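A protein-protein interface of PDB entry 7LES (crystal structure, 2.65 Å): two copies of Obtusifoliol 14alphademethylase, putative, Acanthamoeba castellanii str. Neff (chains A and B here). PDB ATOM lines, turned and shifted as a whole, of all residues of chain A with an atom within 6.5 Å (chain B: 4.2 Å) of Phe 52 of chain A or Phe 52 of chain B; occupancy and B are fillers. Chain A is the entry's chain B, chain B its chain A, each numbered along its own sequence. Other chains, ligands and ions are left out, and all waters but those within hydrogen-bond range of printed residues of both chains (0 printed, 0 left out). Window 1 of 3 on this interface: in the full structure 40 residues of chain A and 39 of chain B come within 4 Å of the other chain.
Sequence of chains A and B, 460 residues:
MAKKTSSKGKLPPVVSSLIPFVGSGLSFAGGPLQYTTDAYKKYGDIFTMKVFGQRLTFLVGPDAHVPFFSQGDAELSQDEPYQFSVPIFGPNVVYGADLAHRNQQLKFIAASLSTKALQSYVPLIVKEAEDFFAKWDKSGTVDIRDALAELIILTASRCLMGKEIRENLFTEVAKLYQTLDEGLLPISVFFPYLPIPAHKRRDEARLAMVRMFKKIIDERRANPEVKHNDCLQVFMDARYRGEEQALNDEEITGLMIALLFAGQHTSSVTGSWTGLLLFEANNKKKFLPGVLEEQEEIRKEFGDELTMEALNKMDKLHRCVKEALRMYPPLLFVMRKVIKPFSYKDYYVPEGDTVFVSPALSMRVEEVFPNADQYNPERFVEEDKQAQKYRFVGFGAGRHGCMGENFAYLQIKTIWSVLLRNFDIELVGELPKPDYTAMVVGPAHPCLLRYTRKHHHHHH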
ATOM      1  N   SER A  17     -18.140  23.933 -15.633  1.00  0.00           N
ATOM      2  CA  SER A  17     -17.004  24.494 -16.365  1.00  0.00           C
ATOM      3  C   SER A  17     -17.039  23.898 -17.763  1.00  0.00           C
ATOM      4  O   SER A  17     -16.707  22.727 -17.943  1.00  0.00           O
ATOM      5  CB  SER A  17     -15.679  24.137 -15.688  1.00  0.00           C
ATOM      6  OG  SER A  17     -15.665  24.547 -14.333  1.00  0.00           O
ATOM      7  N   LEU A  18     -17.438  24.709 -18.741  1.00  0.00           N
ATOM      8  CA  LEU A  18     -17.658  24.254 -20.104  1.00  0.00           C
ATOM      9  C   LEU A  18     -16.530  24.795 -20.996  1.00  0.00           C
ATOM     10  O   LEU A  18     -16.048  25.922 -20.799  1.00  0.00           O
ATOM     11  CB  LEU A  18     -19.043  24.737 -20.552  1.00  0.00           C
ATOM     12  CG  LEU A  18     -20.194  24.511 -19.540  1.00  0.00           C
ATOM     13  CD1 LEU A  18     -21.512  25.141 -20.005  1.00  0.00           C
ATOM     14  CD2 LEU A  18     -20.354  23.024 -19.227  1.00  0.00           C
ATOM     15  N   ILE A  19     -16.068  23.956 -21.926  1.00  0.00           N
ATOM     16  CA  ILE A  19     -15.023  24.324 -22.901  1.00  0.00           C
ATOM     17  C   ILE A  19     -15.452  23.781 -24.258  1.00  0.00           C
ATOM     18  O   ILE A  19     -15.038  22.707 -24.666  1.00  0.00           O
ATOM     19  CB  ILE A  19     -13.617  23.782 -22.526  1.00  0.00           C
ATOM     20  CG1 ILE A  19     -13.334  23.991 -21.024  1.00  0.00           C
ATOM     21  CG2 ILE A  19     -12.552  24.460 -23.389  1.00  0.00           C
ATOM     22  CD1 ILE A  19     -11.922  23.678 -20.576  1.00  0.00           C
ATOM     23  N   PRO A  20     -16.295  24.532 -24.968  1.00  0.00           N
ATOM     24  CA  PRO A  20     -16.840  24.000 -26.198  1.00  0.00           C
ATOM     25  C   PRO A  20     -15.835  24.004 -27.335  1.00  0.00           C
ATOM     26  O   PRO A  20     -14.889  24.786 -27.342  1.00  0.00           O
ATOM     27  CB  PRO A  20     -17.998  24.945 -26.490  1.00  0.00           C
ATOM     28  CG  PRO A  20     -17.585  26.241 -25.893  1.00  0.00           C
ATOM     29  CD  PRO A  20     -16.720  25.923 -24.725  1.00  0.00           C
ATOM     30  N   PHE A  21     -16.052  23.119 -28.287  1.00  0.00           N
ATOM     31  CA  PHE A  21     -15.251  23.072 -29.492  1.00  0.00           C
ATOM     32  C   PHE A  21     -15.507  24.319 -30.354  1.00  0.00           C
ATOM     33  O   PHE A  21     -16.602  24.520 -30.878  1.00  0.00           O
ATOM     34  CB  PHE A  21     -15.627  21.822 -30.255  1.00  0.00           C
ATOM     35  CG  PHE A  21     -14.918  21.662 -31.550  1.00  0.00           C
ATOM     36  CD1 PHE A  21     -13.661  21.055 -31.599  1.00  0.00           C
ATOM     37  CD2 PHE A  21     -15.505  22.071 -32.717  1.00  0.00           C
ATOM     38  CE1 PHE A  21     -13.008  20.861 -32.796  1.00  0.00           C
ATOM     39  CE2 PHE A  21     -14.851  21.891 -33.918  1.00  0.00           C
ATOM     40  CZ  PHE A  21     -13.608  21.280 -33.960  1.00  0.00           C
ATOM     41  N   VAL A  22     -14.473  25.131 -30.512  1.00  0.00           N
ATOM     42  CA  VAL A  22     -14.571  26.448 -31.150  1.00  0.00           C
ATOM     43  C   VAL A  22     -14.752  26.401 -32.687  1.00  0.00           C
ATOM     44  O   VAL A  22     -15.374  27.295 -33.267  1.00  0.00           O
ATOM     45  CB  VAL A  22     -13.312  27.267 -30.789  1.00  0.00           C
ATOM     46  CG1 VAL A  22     -13.229  28.571 -31.561  1.00  0.00           C
ATOM     47  CG2 VAL A  22     -13.305  27.551 -29.301  1.00  0.00           C
ATOM     48  N   LYS A  50      -5.221  31.003 -33.192  1.00  0.00           N
ATOM     49  CA  LYS A  50      -5.587  30.606 -31.828  1.00  0.00           C
ATOM     50  C   LYS A  50      -6.836  31.399 -31.486  1.00  0.00           C
ATOM     51  O   LYS A  50      -6.882  32.620 -31.704  1.00  0.00           O
ATOM     52  CB  LYS A  50      -4.477  30.887 -30.814  1.00  0.00           C
ATOM     53  CG  LYS A  50      -3.528  29.713 -30.538  1.00  0.00           C
ATOM     54  CD  LYS A  50      -3.806  28.991 -29.216  1.00  0.00           C
ATOM     55  CE  LYS A  50      -2.566  28.308 -28.645  1.00  0.00           C
ATOM     56  NZ  LYS A  50      -1.519  29.277 -28.195  1.00  0.00           N
ATOM     57  N   VAL A  51      -7.871  30.675 -31.048  1.00  0.00           N
ATOM     58  CA  VAL A  51      -9.059  31.256 -30.455  1.00  0.00           C
ATOM     59  C   VAL A  51      -9.426  30.420 -29.242  1.00  0.00           C
ATOM     60  O   VAL A  51      -9.545  29.219 -29.356  1.00  0.00           O
ATOM     61  CB  VAL A  51     -10.247  31.295 -31.424  1.00  0.00           C
ATOM     62  CG1 VAL A  51     -11.489  31.793 -30.703  1.00  0.00           C
ATOM     63  CG2 VAL A  51      -9.962  32.210 -32.607  1.00  0.00           C
ATOM     64  N   PHE A  52      -9.626  31.076 -28.096  1.00  0.00           N
ATOM     65  CA  PHE A  52      -9.806  30.415 -26.801  1.00  0.00           C
ATOM     66  C   PHE A  52      -8.859  29.220 -26.660  1.00  0.00           C
ATOM     67  O   PHE A  52      -9.272  28.108 -26.318  1.00  0.00           O
ATOM     68  CB  PHE A  52     -11.250  29.975 -26.595  1.00  0.00           C
ATOM     69  CG  PHE A  52     -12.239  31.105 -26.512  1.00  0.00           C
ATOM     70  CD1 PHE A  52     -12.344  31.879 -25.355  1.00  0.00           C
ATOM     71  CD2 PHE A  52     -13.115  31.368 -27.561  1.00  0.00           C
ATOM     72  CE1 PHE A  52     -13.281  32.907 -25.252  1.00  0.00           C
ATOM     73  CE2 PHE A  52     -14.048  32.392 -27.460  1.00  0.00           C
ATOM     74  CZ  PHE A  52     -14.125  33.161 -26.305  1.00  0.00           C
ATOM     75  N   GLY A  53      -7.586  29.455 -26.954  1.00  0.00           N
ATOM     76  CA  GLY A  53      -6.560  28.441 -26.778  1.00  0.00           C
ATOM     77  C   GLY A  53      -6.890  27.185 -27.541  1.00  0.00           C
ATOM     78  O   GLY A  53      -6.751  26.095 -27.000  1.00  0.00           O
ATOM     79  N   GLN A  54      -7.380  27.356 -28.774  1.00  0.00           N
ATOM     80  CA  GLN A  54      -7.649  26.254 -29.703  1.00  0.00           C
ATOM     81  C   GLN A  54      -7.075  26.603 -31.083  1.00  0.00           C
ATOM     82  O   GLN A  54      -7.434  27.621 -31.690  1.00  0.00           O
ATOM     83  CB  GLN A  54      -9.148  25.934 -29.757  1.00  0.00           C
ATOM     84  CG  GLN A  54      -9.616  25.215 -28.504  1.00  0.00           C
ATOM     85  CD  GLN A  54     -11.116  25.045 -28.417  1.00  0.00           C
ATOM     86  OE1 GLN A  54     -11.768  24.758 -29.410  1.00  0.00           O
ATOM     87  NE2 GLN A  54     -11.675  25.219 -27.218  1.00  0.00           N
ATOM     88  N   PHE A 190     -22.180  25.042 -30.381  1.00  0.00           N
ATOM     89  CA  PHE A 190     -21.314  24.933 -29.219  1.00  0.00           C
ATOM     90  C   PHE A 190     -22.004  24.087 -28.123  1.00  0.00           C
ATOM     91  O   PHE A 190     -21.376  23.198 -27.554  1.00  0.00           O
ATOM     92  CB  PHE A 190     -20.904  26.319 -28.706  1.00  0.00           C
ATOM     93  CG  PHE A 190     -20.281  27.224 -29.747  1.00  0.00           C
ATOM     94  CD1 PHE A 190     -18.923  27.239 -29.954  1.00  0.00           C
ATOM     95  CD2 PHE A 190     -21.062  28.124 -30.476  1.00  0.00           C
ATOM     96  CE1 PHE A 190     -18.346  28.101 -30.902  1.00  0.00           C
ATOM     97  CE2 PHE A 190     -20.493  28.997 -31.420  1.00  0.00           C
ATOM     98  CZ  PHE A 190     -19.126  28.984 -31.638  1.00  0.00           C
ATOM     99  N   LEU B  18      -6.338  35.081 -30.039  1.00  0.00           N
ATOM    100  CA  LEU B  18      -7.384  35.893 -29.438  1.00  0.00           C
ATOM    101  C   LEU B  18      -8.114  35.109 -28.381  1.00  0.00           C
ATOM    102  O   LEU B  18      -8.350  33.901 -28.558  1.00  0.00           O
ATOM    103  CB  LEU B  18      -8.360  36.287 -30.515  1.00  0.00           C
ATOM    104  CG  LEU B  18      -7.747  37.059 -31.684  1.00  0.00           C
ATOM    105  CD1 LEU B  18      -8.800  37.328 -32.749  1.00  0.00           C
ATOM    106  CD2 LEU B  18      -7.108  38.369 -31.232  1.00  0.00           C
ATOM    107  N   ILE B  19      -8.421  35.803 -27.272  1.00  0.00           N
ATOM    108  CA  ILE B  19      -9.287  35.293 -26.199  1.00  0.00           C
ATOM    109  C   ILE B  19     -10.289  36.407 -25.844  1.00  0.00           C
ATOM    110  O   ILE B  19     -10.038  37.197 -24.946  1.00  0.00           O
ATOM    111  CB  ILE B  19      -8.472  34.857 -24.959  1.00  0.00           C
ATOM    112  CG1 ILE B  19      -7.473  33.761 -25.356  1.00  0.00           C
ATOM    113  CG2 ILE B  19      -9.387  34.360 -23.820  1.00  0.00           C
ATOM    114  CD1 ILE B  19      -6.621  33.248 -24.206  1.00  0.00           C
ATOM    115  N   PRO B  20     -11.433  36.476 -26.540  1.00  0.00           N
ATOM    116  CA  PRO B  20     -12.335  37.591 -26.296  1.00  0.00           C
ATOM    117  C   PRO B  20     -13.129  37.461 -24.997  1.00  0.00           C
ATOM    118  O   PRO B  20     -13.085  36.410 -24.316  1.00  0.00           O
ATOM    119  CB  PRO B  20     -13.271  37.551 -27.500  1.00  0.00           C
ATOM    120  CG  PRO B  20     -13.321  36.112 -27.877  1.00  0.00           C
ATOM    121  CD  PRO B  20     -12.006  35.504 -27.485  1.00  0.00           C
ATOM    122  N   VAL B  22     -16.034  36.663 -22.980  1.00  0.00           N
ATOM    123  CA  VAL B  22     -17.023  35.643 -23.259  1.00  0.00           C
ATOM    124  C   VAL B  22     -18.428  36.047 -22.826  1.00  0.00           C
ATOM    125  O   VAL B  22     -19.406  35.677 -23.461  1.00  0.00           O
ATOM    126  CB  VAL B  22     -16.602  34.305 -22.640  1.00  0.00           C
ATOM    127  CG1 VAL B  22     -16.881  34.259 -21.154  1.00  0.00           C
ATOM    128  CG2 VAL B  22     -17.310  33.166 -23.339  1.00  0.00           C
ATOM    129  N   VAL B  51     -16.875  29.478 -18.532  1.00  0.00           N
ATOM    130  CA  VAL B  51     -16.836  29.164 -19.947  1.00  0.00           C
ATOM    131  C   VAL B  51     -15.448  29.581 -20.418  1.00  0.00           C
ATOM    132  O   VAL B  51     -15.081  30.755 -20.241  1.00  0.00           O
ATOM    133  CB  VAL B  51     -17.911  29.946 -20.717  1.00  0.00           C
ATOM    134  CG1 VAL B  51     -17.883  29.588 -22.197  1.00  0.00           C
ATOM    135  CG2 VAL B  51     -19.278  29.648 -20.144  1.00  0.00           C
ATOM    136  N   PHE B  52     -14.683  28.641 -20.999  1.00  0.00           N
ATOM    137  CA  PHE B  52     -13.286  28.901 -21.404  1.00  0.00           C
ATOM    138  C   PHE B  52     -12.547  29.540 -20.226  1.00  0.00           C
ATOM    139  O   PHE B  52     -11.853  30.547 -20.378  1.00  0.00           O
ATOM    140  CB  PHE B  52     -13.169  29.857 -22.613  1.00  0.00           C
ATOM    141  CG  PHE B  52     -13.854  29.394 -23.872  1.00  0.00           C
ATOM    142  CD1 PHE B  52     -13.359  28.310 -24.605  1.00  0.00           C
ATOM    143  CD2 PHE B  52     -14.956  30.104 -24.388  1.00  0.00           C
ATOM    144  CE1 PHE B  52     -13.975  27.918 -25.796  1.00  0.00           C
ATOM    145  CE2 PHE B  52     -15.580  29.700 -25.572  1.00  0.00           C
ATOM    146  CZ  PHE B  52     -15.092  28.604 -26.271  1.00  0.00           C
ATOM    147  N   GLY B  53     -12.772  29.006 -19.029  1.00  0.00           N
ATOM    148  CA  GLY B  53     -12.106  29.499 -17.816  1.00  0.00           C
ATOM    149  C   GLY B  53     -12.652  30.765 -17.168  1.00  0.00           C
ATOM    150  O   GLY B  53     -12.428  30.993 -15.950  1.00  0.00           O
ATOM    151  N   GLN B  54     -13.389  31.564 -17.957  1.00  0.00           N
ATOM    152  CA  GLN B  54     -13.851  32.879 -17.531  1.00  0.00           C
ATOM    153  C   GLN B  54     -15.031  32.722 -16.587  1.00  0.00           C
ATOM    154  O   GLN B  54     -15.985  32.022 -16.901  1.00  0.00           O
ATOM    155  CB  GLN B  54     -14.254  33.730 -18.723  1.00  0.00           C
ATOM    156  CG  GLN B  54     -13.160  33.857 -19.748  1.00  0.00           C
ATOM    157  CD  GLN B  54     -13.467  34.865 -20.821  1.00  0.00           C
ATOM    158  OE1 GLN B  54     -14.299  35.737 -20.623  1.00  0.00           O
ATOM    159  NE2 GLN B  54     -12.780  34.750 -21.977  1.00  0.00           N
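O of Lys 50 of chain A sits at hydrogen-bond distance from N of Leu 18 of chain B (3.0 Å).
The backbone carbonyl oxygen of Leu 18 of chain B sits at hydrogen-bond distance from the backbone NH of Phe 52 of chain A (3.1 Å).
The backbone NH of Phe 52 of chain B sits at hydrogen-bond distance from the backbone carbonyl oxygen of Leu 18 of chain A, 3.0 Å away.
O of Pro 20 of chain B is in hydrogen-bond range of NE2 of Gln 54 of chain B, at 2.9 Å.
The side-chain amide oxygen (OE1) of Gln 54 of chain B sits close to the backbone NH (N) of Val 22 of chain B, 3.1 Å away.
The backbone carbonyl oxygen of Pro 20 of chain A is in hydrogen-bond range of the side-chain amide nitrogen of Gln 54 of chain A, 3.2 Å away.
The backbone NH (N) of Val 22 of chain A is in hydrogen-bond range of the side-chain amide oxygen (OE1) of Gln 54 of chain A, 2.9 Å away.
Among the printed residues, pairs that only touch across the chains: Phe 52 of chain A with Phe 52 of chain B, Val 51 of chain A with Leu 18 of chain B, Phe 52 of chain A with Pro 20 of chain B, Leu 18 of chain A with Val 51 of chain B, Pro 20 of chain A with Phe 52 of chain B, Val 22 of chain A with Phe 52 of chain B, Phe 52 of chain A with Gln 54 of chain B and Gln 54 of chain A with Phe 52 of chain B.
Printed residues of chain A within 4 Å of Gln 54 of chain B: Phe 52.
Printed residues of chain B within 4 Å of Gln 54 of chain A: Phe 52 (3.8 Å).
Val 22 of chain B touches none of the printed residues of chain A.
Gly 53 of chain A touches none of the printed residues of chain B.
The nearest printed residue of chain B that does not touch Phe 52 of chain A is Ile 19 of chain B (4.2 Å).
Printed residues of chain A that touch a printed residue of chain B: Leu 18, Pro 20, Val 22, Lys 50, Val 51, Phe 52 and Gln 54.
Hydrophobic or aromatic side chains of chain A within 4 Å of the printed part of chain B: Pro 20, Val 22 and Phe 52.
Hydrophobic or aromatic side chains of chain B within 4 Å of the printed part of chain A: Pro 20 and Phe 52.
Along chain B the printed residues that touch a printed residue of chain A span positions 18 to 54.
Among the printed residues, no Asp or Glu carboxylate lies within 4 Å of a Lys or Arg side-chain nitrogen of the other chain.
Leu 18 of chain A touches Val 51 of chain B, and with the chains exchanged Val 51 of chain A touches Leu 18 of chain B.
Pro 20 of chain A touches Phe 52 of chain B, and with the chains exchanged Phe 52 of chain A touches Pro 20 of chain B.
Phe 52 of chain A touches its own counterpart, Phe 52 of chain B.
Phe 52 of chain A touches Gln 54 of chain B, and with the chains exchanged Gln 54 of chain A touches Phe 52 of chain B.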
